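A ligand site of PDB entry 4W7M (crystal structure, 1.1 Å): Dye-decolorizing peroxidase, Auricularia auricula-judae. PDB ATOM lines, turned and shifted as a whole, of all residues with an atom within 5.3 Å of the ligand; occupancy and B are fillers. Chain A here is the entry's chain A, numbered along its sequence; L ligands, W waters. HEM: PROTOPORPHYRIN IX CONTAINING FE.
A ring nitrogen (NE2) of His 305 is bound to an iron atom (FE) of the ligand, 2.1 Å away. N of Ile 171 is in hydrogen-bond range of O2A of the ligand (2.7 Å). The guanidinium group of Arg 333 lies within salt-bridge range of an oxygen (O2A) of the ligand, at 2.8 Å. The guanidinium group (NH2) of Arg 312 is in salt-bridge range of an oxygen (O1D) of the ligand. The backbone NH of Gly 170 lies within hydrogen-bond range of an oxygen (O2A) of the ligand (3.1 Å). N of Ala 172 lies within hydrogen-bond range of O2A of the ligand (3.2 Å). NE of Arg 256 lies within salt-bridge range of O1A of the ligand (3.5 Å).
The backbone carbonyl oxygen (O) of His 305 lies within hydrogen-bond range of the side-chain hydroxyl (OG1) of Thr 309 (3.2 Å). The backbone carbonyl oxygen (O) of Val 254 is in hydrogen-bond range of the backbone NH (N) of His 305, 3.4 Å away. The side-chain carboxylate (OE1) of Glu 163 sits at hydrogen-bond distance from the backbone NH (N) of Phe 167, 2.8 Å away. The side-chain carboxylate (OE2) of Glu 163 is in hydrogen-bond range of the backbone NH (N) of Phe 165, at 2.8 Å. O of Ile 399 is in hydrogen-bond range of NE2 of Gln 375, 2.9 Å away. OD1 of Asn 282 is in hydrogen-bond range of NH2 of Arg 256, 3.0 Å away. O of Leu 220 sits at hydrogen-bond distance from N of Leu 358. The backbone carbonyl oxygen (O) of Val 254 lies within hydrogen-bond range of the backbone NH (N) of Ile 306, 3.0 Å away.
Merely in contact with the ligand: Thr 309, Phe 360, Glu 163, Arg 310, Gln 222, Leu 168, Phe 167, Ile 399, Phe 371, Asp 169, Leu 358, Ile 306, Gln 375, Leu 220, Val 427, Leu 374, Val 254 and Ile 331. Hydrophobic or aromatic side chains that line the ligand: Phe 167, Ile 171, Ala 172, Leu 220, Val 254, His 305, Ile 306, Ile 331, Leu 358, Phe 360, Phe 371, Leu 374, Ile 399 and Val 427. 25 residues have an atom within 4 Å of the ligand: Glu 163, Phe 167, Leu 168, Asp 169, Gly 170, Ile 171, Ala 172, Leu 220, Gln 222, Val 254, Arg 256, His 305, Ile 306, Thr 309, Arg 310, Arg 312, Ile 331, Arg 333, Leu 358, Phe 360, Phe 371, Leu 374, Gln 375, Ile 399 and Val 427. Along chain A the residues within 4 Å of the ligand span positions 163 to 427.
Water W1 lies within hydrogen-bond range of O1A of the ligand and NH2 of Arg 256. Water W2 lies within hydrogen-bond range of the backbone carbonyl oxygen (O) of Arg 310 (2.7 Å), the side-chain hydroxyl (OH) of Tyr 286 (2.7 Å), an oxygen (O1D) of the ligand (2.8 Å), the guanidinium group (NE) of Arg 312 (2.8 Å) and the backbone carbonyl oxygen (O) of Ile 306 (2.9 Å).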
ATOM      1  N   GLU A 163     -21.018 -29.330  28.884  1.00  0.00           N
ATOM      2  CA  GLU A 163     -21.348 -27.915  28.941  1.00  0.00           C
ATOM      3  C   GLU A 163     -22.685 -27.670  28.217  1.00  0.00           C
ATOM      4  O   GLU A 163     -23.302 -28.590  27.704  1.00  0.00           O
ATOM      5  CB  GLU A 163     -20.166 -27.054  28.447  1.00  0.00           C
ATOM      6  CG  GLU A 163     -19.611 -27.415  27.108  1.00  0.00           C
ATOM      7  CD  GLU A 163     -20.604 -27.105  26.020  1.00  0.00           C
ATOM      8  OE1 GLU A 163     -20.940 -28.011  25.232  1.00  0.00           O
ATOM      9  OE2 GLU A 163     -21.082 -25.939  25.987  1.00  0.00           O
ATOM     10  N   PHE A 165     -23.753 -26.371  25.420  1.00  0.00           N
ATOM     11  CA  PHE A 165     -23.971 -26.762  24.027  1.00  0.00           C
ATOM     12  C   PHE A 165     -24.107 -28.286  23.869  1.00  0.00           C
ATOM     13  O   PHE A 165     -24.431 -28.747  22.775  1.00  0.00           O
ATOM     14  CB  PHE A 165     -22.822 -26.299  23.112  1.00  0.00           C
ATOM     15  CG  PHE A 165     -22.739 -24.801  22.893  1.00  0.00           C
ATOM     16  CD1 PHE A 165     -23.861 -24.020  22.748  1.00  0.00           C
ATOM     17  CD2 PHE A 165     -21.488 -24.193  22.789  1.00  0.00           C
ATOM     18  CE1 PHE A 165     -23.745 -22.650  22.536  1.00  0.00           C
ATOM     19  CE2 PHE A 165     -21.373 -22.833  22.580  1.00  0.00           C
ATOM     20  CZ  PHE A 165     -22.501 -22.064  22.462  1.00  0.00           C
ATOM     21  N   PHE A 167     -21.540 -30.683  24.820  1.00  0.00           N
ATOM     22  CA  PHE A 167     -20.280 -31.405  24.640  1.00  0.00           C
ATOM     23  C   PHE A 167     -19.665 -31.780  25.971  1.00  0.00           C
ATOM     24  O   PHE A 167     -19.588 -30.965  26.882  1.00  0.00           O
ATOM     25  CB  PHE A 167     -19.284 -30.555  23.844  1.00  0.00           C
ATOM     26  CG  PHE A 167     -19.690 -30.305  22.419  1.00  0.00           C
ATOM     27  CD1 PHE A 167     -20.651 -29.346  22.121  1.00  0.00           C
ATOM     28  CD2 PHE A 167     -19.148 -31.021  21.375  1.00  0.00           C
ATOM     29  CE1 PHE A 167     -21.086 -29.140  20.823  1.00  0.00           C
ATOM     30  CE2 PHE A 167     -19.549 -30.822  20.066  1.00  0.00           C
ATOM     31  CZ  PHE A 167     -20.523 -29.866  19.787  1.00  0.00           C
ATOM     32  N   LEU A 168     -19.208 -33.023  26.057  1.00  0.00           N
ATOM     33  CA  LEU A 168     -18.493 -33.484  27.234  1.00  0.00           C
ATOM     34  C   LEU A 168     -17.298 -32.560  27.446  1.00  0.00           C
ATOM     35  O   LEU A 168     -16.529 -32.274  26.524  1.00  0.00           O
ATOM     36  CB  LEU A 168     -18.022 -34.928  27.060  1.00  0.00           C
ATOM     37  CG  LEU A 168     -17.319 -35.535  28.271  1.00  0.00           C
ATOM     38  CD1 LEU A 168     -18.229 -35.586  29.484  1.00  0.00           C
ATOM     39  CD2 LEU A 168     -16.806 -36.931  27.952  1.00  0.00           C
ATOM     40  N   ASP A 169     -17.134 -32.117  28.671  1.00  0.00           N
ATOM     41  CA  ASP A 169     -16.113 -31.157  29.011  1.00  0.00           C
ATOM     42  C   ASP A 169     -15.248 -31.725  30.135  1.00  0.00           C
ATOM     43  O   ASP A 169     -15.600 -32.739  30.730  1.00  0.00           O
ATOM     44  CB  ASP A 169     -16.808 -29.857  29.433  1.00  0.00           C
ATOM     45  CG  ASP A 169     -15.874 -28.665  29.524  1.00  0.00           C
ATOM     46  OD1 ASP A 169     -14.728 -28.705  29.010  1.00  0.00           O
ATOM     47  OD2 ASP A 169     -16.343 -27.652  30.100  1.00  0.00           O
ATOM     48  N   GLY A 170     -14.120 -31.095  30.391  1.00  0.00           N
ATOM     49  CA  GLY A 170     -13.216 -31.549  31.449  1.00  0.00           C
ATOM     50  C   GLY A 170     -12.348 -32.748  31.085  1.00  0.00           C
ATOM     51  O   GLY A 170     -11.804 -33.410  31.964  1.00  0.00           O
ATOM     52  N   ILE A 171     -12.205 -33.016  29.797  1.00  0.00           N
ATOM     53  CA  ILE A 171     -11.425 -34.142  29.322  1.00  0.00           C
ATOM     54  C   ILE A 171      -9.933 -33.828  29.387  1.00  0.00           C
ATOM     55  O   ILE A 171      -9.140 -34.603  29.934  1.00  0.00           O
ATOM     56  CB  ILE A 171     -11.809 -34.506  27.880  1.00  0.00           C
ATOM     57  CG1 ILE A 171     -13.267 -34.972  27.807  1.00  0.00           C
ATOM     58  CG2 ILE A 171     -10.868 -35.566  27.335  1.00  0.00           C
ATOM     59  CD1 ILE A 171     -13.797 -35.081  26.392  1.00  0.00           C
ATOM     60  N   ALA A 172      -9.553 -32.694  28.821  1.00  0.00           N
ATOM     61  CA  ALA A 172      -8.155 -32.388  28.562  1.00  0.00           C
ATOM     62  C   ALA A 172      -7.598 -31.356  29.557  1.00  0.00           C
ATOM     63  O   ALA A 172      -8.111 -30.246  29.678  1.00  0.00           O
ATOM     64  CB  ALA A 172      -7.991 -31.873  27.129  1.00  0.00           C
ATOM     65  N   GLN A 173      -6.529 -31.718  30.234  1.00  0.00           N
ATOM     66  CA  GLN A 173      -5.816 -30.833  31.141  1.00  0.00           C
ATOM     67  C   GLN A 173      -4.336 -31.121  30.998  1.00  0.00           C
ATOM     68  O   GLN A 173      -3.950 -32.245  30.663  1.00  0.00           O
ATOM     69  CB  GLN A 173      -6.190 -31.121  32.590  1.00  0.00           C
ATOM     70  CG  GLN A 173      -7.658 -31.076  32.914  1.00  0.00           C
ATOM     71  CD  GLN A 173      -8.245 -29.683  33.082  1.00  0.00           C
ATOM     72  OE1 GLN A 173      -7.650 -28.661  32.728  1.00  0.00           O
ATOM     73  NE2 GLN A 173      -9.449 -29.654  33.608  1.00  0.00           N
ATOM     74  N   LEU A 220     -19.413 -16.473  30.693  1.00  0.00           N
ATOM     75  CA  LEU A 220     -19.600 -16.621  29.245  1.00  0.00           C
ATOM     76  C   LEU A 220     -20.978 -17.181  28.912  1.00  0.00           C
ATOM     77  O   LEU A 220     -21.238 -18.370  29.075  1.00  0.00           O
ATOM     78  CB  LEU A 220     -18.496 -17.529  28.679  1.00  0.00           C
ATOM     79  CG  LEU A 220     -17.066 -17.033  28.919  1.00  0.00           C
ATOM     80  CD1 LEU A 220     -16.040 -17.985  28.347  1.00  0.00           C
ATOM     81  CD2 LEU A 220     -16.852 -15.647  28.326  1.00  0.00           C
ATOM     82  N   GLN A 222     -23.939 -18.554  26.716  1.00  0.00           N
ATOM     83  CA  GLN A 222     -24.027 -19.384  25.523  1.00  0.00           C
ATOM     84  C   GLN A 222     -25.434 -19.294  24.962  1.00  0.00           C
ATOM     85  O   GLN A 222     -26.396 -19.435  25.690  1.00  0.00           O
ATOM     86  CB  GLN A 222     -23.687 -20.826  25.857  1.00  0.00           C
ATOM     87  CG  GLN A 222     -22.233 -20.966  26.262  1.00  0.00           C
ATOM     88  CD  GLN A 222     -21.890 -22.333  26.782  1.00  0.00           C
ATOM     89  OE1 GLN A 222     -21.689 -22.532  27.973  1.00  0.00           O
ATOM     90  NE2 GLN A 222     -21.793 -23.292  25.877  1.00  0.00           N
ATOM     91  N   VAL A 254     -15.900 -27.714  17.380  1.00  0.00           N
ATOM     92  CA  VAL A 254     -15.303 -27.903  18.695  1.00  0.00           C
ATOM     93  C   VAL A 254     -13.957 -28.636  18.586  1.00  0.00           C
ATOM     94  O   VAL A 254     -13.021 -28.364  19.343  1.00  0.00           O
ATOM     95  CB  VAL A 254     -16.280 -28.675  19.622  1.00  0.00           C
ATOM     96  CG1 VAL A 254     -15.634 -29.060  20.930  1.00  0.00           C
ATOM     97  CG2 VAL A 254     -17.498 -27.821  19.879  1.00  0.00           C
ATOM     98  N   ARG A 256     -14.220 -32.021  18.935  1.00  0.00           N
ATOM     99  CA  ARG A 256     -14.701 -33.264  19.515  1.00  0.00           C
ATOM    100  C   ARG A 256     -16.176 -33.393  19.222  1.00  0.00           C
ATOM    101  O   ARG A 256     -16.876 -32.389  19.154  1.00  0.00           O
ATOM    102  CB  ARG A 256     -14.541 -33.301  21.038  1.00  0.00           C
ATOM    103  CG  ARG A 256     -13.109 -33.260  21.517  1.00  0.00           C
ATOM    104  CD  ARG A 256     -13.044 -33.419  23.050  1.00  0.00           C
ATOM    105  NE  ARG A 256     -11.652 -33.382  23.499  1.00  0.00           N
ATOM    106  CZ  ARG A 256     -10.828 -34.419  23.504  1.00  0.00           C
ATOM    107  NH1 ARG A 256     -11.263 -35.640  23.222  1.00  0.00           N
ATOM    108  NH2 ARG A 256      -9.566 -34.252  23.842  1.00  0.00           N
ATOM    109  N   ASN A 282      -7.615 -38.769  24.214  1.00  0.00           N
ATOM    110  CA  ASN A 282      -6.691 -37.630  24.077  1.00  0.00           C
ATOM    111  C   ASN A 282      -5.428 -38.005  23.316  1.00  0.00           C
ATOM    112  O   ASN A 282      -4.521 -37.190  23.208  1.00  0.00           O
ATOM    113  CB  ASN A 282      -6.348 -37.001  25.440  1.00  0.00           C
ATOM    114  CG  ASN A 282      -6.207 -35.497  25.344  1.00  0.00           C
ATOM    115  OD1 ASN A 282      -6.695 -34.892  24.398  1.00  0.00           O
ATOM    116  ND2 ASN A 282      -5.538 -34.893  26.311  1.00  0.00           N
ATOM    117  N   TYR A 286      -2.664 -34.241  15.974  1.00  0.00           N
ATOM    118  CA  TYR A 286      -3.099 -33.619  14.705  1.00  0.00           C
ATOM    119  C   TYR A 286      -2.283 -34.052  13.480  1.00  0.00           C
ATOM    120  O   TYR A 286      -2.673 -33.763  12.345  1.00  0.00           O
ATOM    121  CB  TYR A 286      -3.222 -32.079  14.772  1.00  0.00           C
ATOM    122  CG  TYR A 286      -4.238 -31.638  15.796  1.00  0.00           C
ATOM    123  CD1 TYR A 286      -5.550 -32.089  15.727  1.00  0.00           C
ATOM    124  CD2 TYR A 286      -3.884 -30.804  16.853  1.00  0.00           C
ATOM    125  CE1 TYR A 286      -6.475 -31.717  16.690  1.00  0.00           C
ATOM    126  CE2 TYR A 286      -4.805 -30.445  17.810  1.00  0.00           C
ATOM    127  CZ  TYR A 286      -6.096 -30.901  17.732  1.00  0.00           C
ATOM    128  OH  TYR A 286      -7.051 -30.564  18.671  1.00  0.00           O
ATOM    129  N   HIS A 305     -12.025 -25.396  17.976  1.00  0.00           N
ATOM    130  CA  HIS A 305     -11.740 -24.836  19.293  1.00  0.00           C
ATOM    131  C   HIS A 305     -10.549 -25.503  19.981  1.00  0.00           C
ATOM    132  O   HIS A 305      -9.634 -24.810  20.444  1.00  0.00           O
ATOM    133  CB  HIS A 305     -12.989 -24.924  20.160  1.00  0.00           C
ATOM    134  CG  HIS A 305     -12.799 -24.434  21.561  1.00  0.00           C
ATOM    135  ND1 HIS A 305     -12.338 -23.176  21.838  1.00  0.00           N
ATOM    136  CD2 HIS A 305     -13.049 -25.015  22.766  1.00  0.00           C
ATOM    137  CE1 HIS A 305     -12.305 -23.004  23.155  1.00  0.00           C
ATOM    138  NE2 HIS A 305     -12.728 -24.107  23.740  1.00  0.00           N
ATOM    139  N   ILE A 306     -10.553 -26.827  20.105  1.00  0.00           N
ATOM    140  CA  ILE A 306      -9.461 -27.434  20.851  1.00  0.00           C
ATOM    141  C   ILE A 306      -8.128 -27.359  20.122  1.00  0.00           C
ATOM    142  O   ILE A 306      -7.070 -27.342  20.766  1.00  0.00           O
ATOM    143  CB  ILE A 306      -9.758 -28.884  21.295  1.00  0.00           C
ATOM    144  CG1 ILE A 306      -9.913 -29.846  20.126  1.00  0.00           C
ATOM    145  CG2 ILE A 306     -10.976 -28.928  22.183  1.00  0.00           C
ATOM    146  CD1 ILE A 306      -9.733 -31.309  20.540  1.00  0.00           C
ATOM    147  N   THR A 309      -6.831 -23.947  21.032  1.00  0.00           N
ATOM    148  CA  THR A 309      -6.434 -23.739  22.411  1.00  0.00           C
ATOM    149  C   THR A 309      -5.306 -24.669  22.882  1.00  0.00           C
ATOM    150  O   THR A 309      -4.641 -24.339  23.842  1.00  0.00           O
ATOM    151  CB  THR A 309      -7.616 -23.823  23.356  1.00  0.00           C
ATOM    152  OG1 THR A 309      -8.201 -25.114  23.247  1.00  0.00           O
ATOM    153  CG2 THR A 309      -8.650 -22.721  23.053  1.00  0.00           C
ATOM    154  N   ARG A 310      -5.115 -25.793  22.207  1.00  0.00           N
ATOM    155  CA  ARG A 310      -3.898 -26.623  22.365  1.00  0.00           C
ATOM    156  C   ARG A 310      -3.483 -27.118  20.979  1.00  0.00           C
ATOM    157  O   ARG A 310      -3.962 -28.150  20.497  1.00  0.00           O
ATOM    158  CB  ARG A 310      -4.077 -27.806  23.320  1.00  0.00           C
ATOM    159  CG  ARG A 310      -2.763 -28.558  23.539  1.00  0.00           C
ATOM    160  CD  ARG A 310      -2.906 -29.884  24.298  1.00  0.00           C
ATOM    161  NE  ARG A 310      -1.644 -30.605  24.199  1.00  0.00           N
ATOM    162  CZ  ARG A 310      -1.508 -31.921  24.337  1.00  0.00           C
ATOM    163  NH1 ARG A 310      -2.531 -32.697  24.644  1.00  0.00           N
ATOM    164  NH2 ARG A 310      -0.319 -32.469  24.114  1.00  0.00           N
ATOM    165  N   ARG A 312      -0.910 -28.528  19.730  1.00  0.00           N
ATOM    166  CA  ARG A 312      -0.152 -29.773  19.601  1.00  0.00           C
ATOM    167  C   ARG A 312       0.883 -29.663  18.464  1.00  0.00           C
ATOM    168  O   ARG A 312       1.703 -28.752  18.477  1.00  0.00           O
ATOM    169  CB  ARG A 312      -1.083 -31.001  19.460  1.00  0.00           C
ATOM    170  CG  ARG A 312      -2.105 -31.062  20.590  1.00  0.00           C
ATOM    171  CD  ARG A 312      -2.963 -32.332  20.589  1.00  0.00           C
ATOM    172  NE  ARG A 312      -4.108 -32.132  21.483  1.00  0.00           N
ATOM    173  CZ  ARG A 312      -4.651 -33.063  22.255  1.00  0.00           C
ATOM    174  NH1 ARG A 312      -4.215 -34.322  22.237  1.00  0.00           N
ATOM    175  NH2 ARG A 312      -5.666 -32.730  23.042  1.00  0.00           N
ATOM    176  N   ILE A 331      -3.342 -24.168  30.441  1.00  0.00           N
ATOM    177  CA  ILE A 331      -4.191 -23.759  31.530  1.00  0.00           C
ATOM    178  C   ILE A 331      -4.878 -24.968  32.146  1.00  0.00           C
ATOM    179  O   ILE A 331      -5.162 -25.944  31.465  1.00  0.00           O
ATOM    180  CB  ILE A 331      -5.249 -22.715  31.084  1.00  0.00           C
ATOM    181  CG1 ILE A 331      -6.191 -23.276  30.006  1.00  0.00           C
ATOM    182  CG2 ILE A 331      -4.574 -21.424  30.640  1.00  0.00           C
ATOM    183  CD1 ILE A 331      -7.362 -22.369  29.695  1.00  0.00           C
ATOM    184  N   ARG A 333      -8.388 -25.998  33.733  1.00  0.00           N
ATOM    185  CA  ARG A 333      -9.753 -25.502  33.664  1.00  0.00           C
ATOM    186  C   ARG A 333     -10.630 -26.133  34.724  1.00  0.00           C
ATOM    187  O   ARG A 333     -10.629 -27.361  34.895  1.00  0.00           O
ATOM    188  CB  ARG A 333     -10.340 -25.773  32.278  1.00  0.00           C
ATOM    189  CG  ARG A 333      -9.625 -24.997  31.182  1.00  0.00           C
ATOM    190  CD  ARG A 333     -10.143 -25.329  29.795  1.00  0.00           C
ATOM    191  NE  ARG A 333      -9.930 -26.748  29.527  1.00  0.00           N
ATOM    192  CZ  ARG A 333     -10.844 -27.632  29.204  1.00  0.00           C
ATOM    193  NH1 ARG A 333     -12.111 -27.292  28.991  1.00  0.00           N
ATOM    194  NH2 ARG A 333     -10.490 -28.897  29.096  1.00  0.00           N
ATOM    195  N   LEU A 358     -21.326 -20.769  30.613  1.00  0.00           N
ATOM    196  CA  LEU A 358     -20.210 -21.372  31.310  1.00  0.00           C
ATOM    197  C   LEU A 358     -19.609 -20.361  32.282  1.00  0.00           C
ATOM    198  O   LEU A 358     -19.251 -19.251  31.882  1.00  0.00           O
ATOM    199  CB  LEU A 358     -19.134 -21.820  30.323  1.00  0.00           C
ATOM    200  CG  LEU A 358     -17.935 -22.558  30.911  1.00  0.00           C
ATOM    201  CD1 LEU A 358     -18.352 -23.911  31.503  1.00  0.00           C
ATOM    202  CD2 LEU A 358     -16.870 -22.743  29.855  1.00  0.00           C
ATOM    203  N   PHE A 360     -16.568 -19.851  33.498  1.00  0.00           N
ATOM    204  CA  PHE A 360     -15.264 -20.286  33.058  1.00  0.00           C
ATOM    205  C   PHE A 360     -14.224 -19.921  34.114  1.00  0.00           C
ATOM    206  O   PHE A 360     -14.181 -18.775  34.594  1.00  0.00           O
ATOM    207  CB  PHE A 360     -14.953 -19.627  31.713  1.00  0.00           C
ATOM    208  CG  PHE A 360     -13.550 -19.846  31.229  1.00  0.00           C
ATOM    209  CD1 PHE A 360     -12.539 -18.972  31.593  1.00  0.00           C
ATOM    210  CD2 PHE A 360     -13.239 -20.937  30.424  1.00  0.00           C
ATOM    211  CE1 PHE A 360     -11.244 -19.161  31.133  1.00  0.00           C
ATOM    212  CE2 PHE A 360     -11.943 -21.116  29.961  1.00  0.00           C
ATOM    213  CZ  PHE A 360     -10.954 -20.241  30.321  1.00  0.00           C
ATOM    214  N   PHE A 371      -4.595 -17.875  29.832  1.00  0.00           N
ATOM    215  CA  PHE A 371      -5.866 -17.398  29.325  1.00  0.00           C
ATOM    216  C   PHE A 371      -5.742 -16.256  28.315  1.00  0.00           C
ATOM    217  O   PHE A 371      -6.343 -16.278  27.249  1.00  0.00           O
ATOM    218  CB  PHE A 371      -6.794 -16.985  30.469  1.00  0.00           C
ATOM    219  CG  PHE A 371      -7.942 -16.136  30.000  1.00  0.00           C
ATOM    220  CD1 PHE A 371      -8.957 -16.694  29.234  1.00  0.00           C
ATOM    221  CD2 PHE A 371      -7.965 -14.779  30.240  1.00  0.00           C
ATOM    222  CE1 PHE A 371      -9.971 -15.908  28.747  1.00  0.00           C
ATOM    223  CE2 PHE A 371      -8.980 -13.992  29.753  1.00  0.00           C
ATOM    224  CZ  PHE A 371      -9.987 -14.549  28.994  1.00  0.00           C
ATOM    225  N   LEU A 374      -4.312 -17.435  24.971  1.00  0.00           N
ATOM    226  CA  LEU A 374      -5.187 -18.312  24.211  1.00  0.00           C
ATOM    227  C   LEU A 374      -6.318 -17.522  23.577  1.00  0.00           C
ATOM    228  O   LEU A 374      -6.715 -17.817  22.443  1.00  0.00           O
ATOM    229  CB  LEU A 374      -5.693 -19.450  25.077  1.00  0.00           C
ATOM    230  CG  LEU A 374      -4.597 -20.414  25.562  1.00  0.00           C
ATOM    231  CD1 LEU A 374      -5.182 -21.424  26.517  1.00  0.00           C
ATOM    232  CD2 LEU A 374      -3.893 -21.134  24.422  1.00  0.00           C
ATOM    233  N   GLN A 375      -6.857 -16.546  24.285  1.00  0.00           N
ATOM    234  CA  GLN A 375      -7.937 -15.724  23.746  1.00  0.00           C
ATOM    235  C   GLN A 375      -7.424 -14.784  22.628  1.00  0.00           C
ATOM    236  O   GLN A 375      -7.988 -14.734  21.538  1.00  0.00           O
ATOM    237  CB  GLN A 375      -8.618 -14.915  24.844  1.00  0.00           C
ATOM    238  CG  GLN A 375      -9.865 -14.165  24.387  1.00  0.00           C
ATOM    239  CD  GLN A 375     -11.030 -15.107  24.086  1.00  0.00           C
ATOM    240  OE1 GLN A 375     -11.427 -15.894  24.946  1.00  0.00           O
ATOM    241  NE2 GLN A 375     -11.568 -15.032  22.875  1.00  0.00           N
ATOM    242  N   ILE A 398     -16.089 -21.113  18.520  1.00  0.00           N
ATOM    243  CA  ILE A 398     -16.722 -21.142  19.812  1.00  0.00           C
ATOM    244  C   ILE A 398     -16.457 -19.842  20.594  1.00  0.00           C
ATOM    245  O   ILE A 398     -17.406 -19.219  21.072  1.00  0.00           O
ATOM    246  CB  ILE A 398     -16.294 -22.386  20.619  1.00  0.00           C
ATOM    247  CG1 ILE A 398     -16.564 -23.662  19.809  1.00  0.00           C
ATOM    248  CG2 ILE A 398     -17.026 -22.452  21.965  1.00  0.00           C
ATOM    249  CD1 ILE A 398     -17.997 -23.858  19.334  1.00  0.00           C
ATOM    250  N   ILE A 399     -15.190 -19.441  20.728  1.00  0.00           N
ATOM    251  CA  ILE A 399     -14.827 -18.310  21.585  1.00  0.00           C
ATOM    252  C   ILE A 399     -14.196 -17.120  20.879  1.00  0.00           C
ATOM    253  O   ILE A 399     -13.919 -16.098  21.497  1.00  0.00           O
ATOM    254  CB  ILE A 399     -13.902 -18.738  22.744  1.00  0.00           C
ATOM    255  CG1 ILE A 399     -12.604 -19.344  22.217  1.00  0.00           C
ATOM    256  CG2 ILE A 399     -14.632 -19.723  23.655  1.00  0.00           C
ATOM    257  CD1 ILE A 399     -11.491 -19.347  23.258  1.00  0.00           C
ATOM    258  N   VAL A 427     -21.180 -17.350  21.890  1.00  0.00           N
ATOM    259  CA  VAL A 427     -20.701 -17.148  23.243  1.00  0.00           C
ATOM    260  C   VAL A 427     -20.531 -15.646  23.410  1.00  0.00           C
ATOM    261  O   VAL A 427     -19.897 -14.982  22.584  1.00  0.00           O
ATOM    262  CB  VAL A 427     -19.359 -17.884  23.491  1.00  0.00           C
ATOM    263  CG1 VAL A 427     -18.823 -17.521  24.882  1.00  0.00           C
ATOM    264  CG2 VAL A 427     -19.551 -19.366  23.352  1.00  0.00           C
HETATM  265  CHA HEM L   1     -11.529 -27.649  25.651  1.00  0.00           C
HETATM  266  CHB HEM L   1     -16.010 -25.826  25.462  1.00  0.00           C
HETATM  267  CHC HEM L   1     -14.249 -21.466  26.701  1.00  0.00           C
HETATM  268  CHD HEM L   1      -9.724 -23.201  26.519  1.00  0.00           C
HETATM  269  C1A HEM L   1     -12.899 -27.555  25.489  1.00  0.00           C
HETATM  270  C2A HEM L   1     -13.809 -28.611  25.115  1.00  0.00           C
HETATM  271  C3A HEM L   1     -15.033 -28.112  25.075  1.00  0.00           C
HETATM  272  C4A HEM L   1     -14.954 -26.709  25.407  1.00  0.00           C
HETATM  273  CMA HEM L   1     -16.342 -28.838  24.739  1.00  0.00           C
HETATM  274  CAA HEM L   1     -13.380 -30.054  24.814  1.00  0.00           C
HETATM  275  CBA HEM L   1     -13.404 -30.933  26.057  1.00  0.00           C
HETATM  276  CGA HEM L   1     -12.090 -30.990  26.771  1.00  0.00           C
HETATM  277  O1A HEM L   1     -11.027 -31.115  26.144  1.00  0.00           O
HETATM  278  O2A HEM L   1     -12.118 -30.927  28.015  1.00  0.00           O
HETATM  279  C1B HEM L   1     -15.912 -24.473  25.775  1.00  0.00           C
HETATM  280  C2B HEM L   1     -17.005 -23.546  25.824  1.00  0.00           C
HETATM  281  C3B HEM L   1     -16.531 -22.346  26.158  1.00  0.00           C
HETATM  282  C4B HEM L   1     -15.107 -22.479  26.352  1.00  0.00           C
HETATM  283  CMB HEM L   1     -18.467 -23.926  25.462  1.00  0.00           C
HETATM  284  CAB HEM L   1     -17.295 -21.034  26.336  1.00  0.00           C
HETATM  285  CBB HEM L   1     -18.579 -20.969  26.732  1.00  0.00           C
HETATM  286  C1C HEM L   1     -12.856 -21.518  26.692  1.00  0.00           C
HETATM  287  C2C HEM L   1     -11.963 -20.380  26.796  1.00  0.00           C
HETATM  288  C3C HEM L   1     -10.709 -20.875  26.712  1.00  0.00           C
HETATM  289  C4C HEM L   1     -10.785 -22.306  26.579  1.00  0.00           C
HETATM  290  CMC HEM L   1     -12.403 -18.933  26.994  1.00  0.00           C
HETATM  291  CAC HEM L   1      -9.377 -20.128  26.766  1.00  0.00           C
HETATM  292  CBC HEM L   1      -9.266 -18.852  26.440  1.00  0.00           C
HETATM  293  C1D HEM L   1      -9.814 -24.563  26.363  1.00  0.00           C
HETATM  294  C2D HEM L   1      -8.691 -25.458  26.405  1.00  0.00           C
HETATM  295  C3D HEM L   1      -9.245 -26.815  26.146  1.00  0.00           C
HETATM  296  C4D HEM L   1     -10.647 -26.623  25.949  1.00  0.00           C
HETATM  297  CMD HEM L   1      -7.230 -25.136  26.708  1.00  0.00           C
HETATM  298  CAD HEM L   1      -8.427 -28.098  26.093  1.00  0.00           C
HETATM  299  CBD HEM L   1      -7.658 -28.188  24.768  1.00  0.00           C
HETATM  300  CGD HEM L   1      -6.757 -29.404  24.728  1.00  0.00           C
HETATM  301  O1D HEM L   1      -6.853 -30.180  23.722  1.00  0.00           O
HETATM  302  O2D HEM L   1      -5.951 -29.608  25.668  1.00  0.00           O
HETATM  303  NA  HEM L   1     -13.628 -26.402  25.675  1.00  0.00           N
HETATM  304  NB  HEM L   1     -14.745 -23.800  26.124  1.00  0.00           N
HETATM  305  NC  HEM L   1     -12.110 -22.675  26.535  1.00  0.00           N
HETATM  306  ND  HEM L   1     -10.962 -25.284  26.112  1.00  0.00           N
HETATM  307 FE   HEM L   1     -12.838 -24.478  25.814  1.00  0.00          FE
HETATM  308  O   HOH W   1      -9.413 -31.426  24.094  1.00  0.00           O
HETATM  309  O   HOH W   2      -5.907 -29.970  21.093  1.00  0.00           O
HETATM  310  O   HOH W   3      -4.819 -32.014  26.140  1.00  0.00           O
HETATM  311  O   HOH W   4      -5.299 -28.424  28.050  1.00  0.00           O
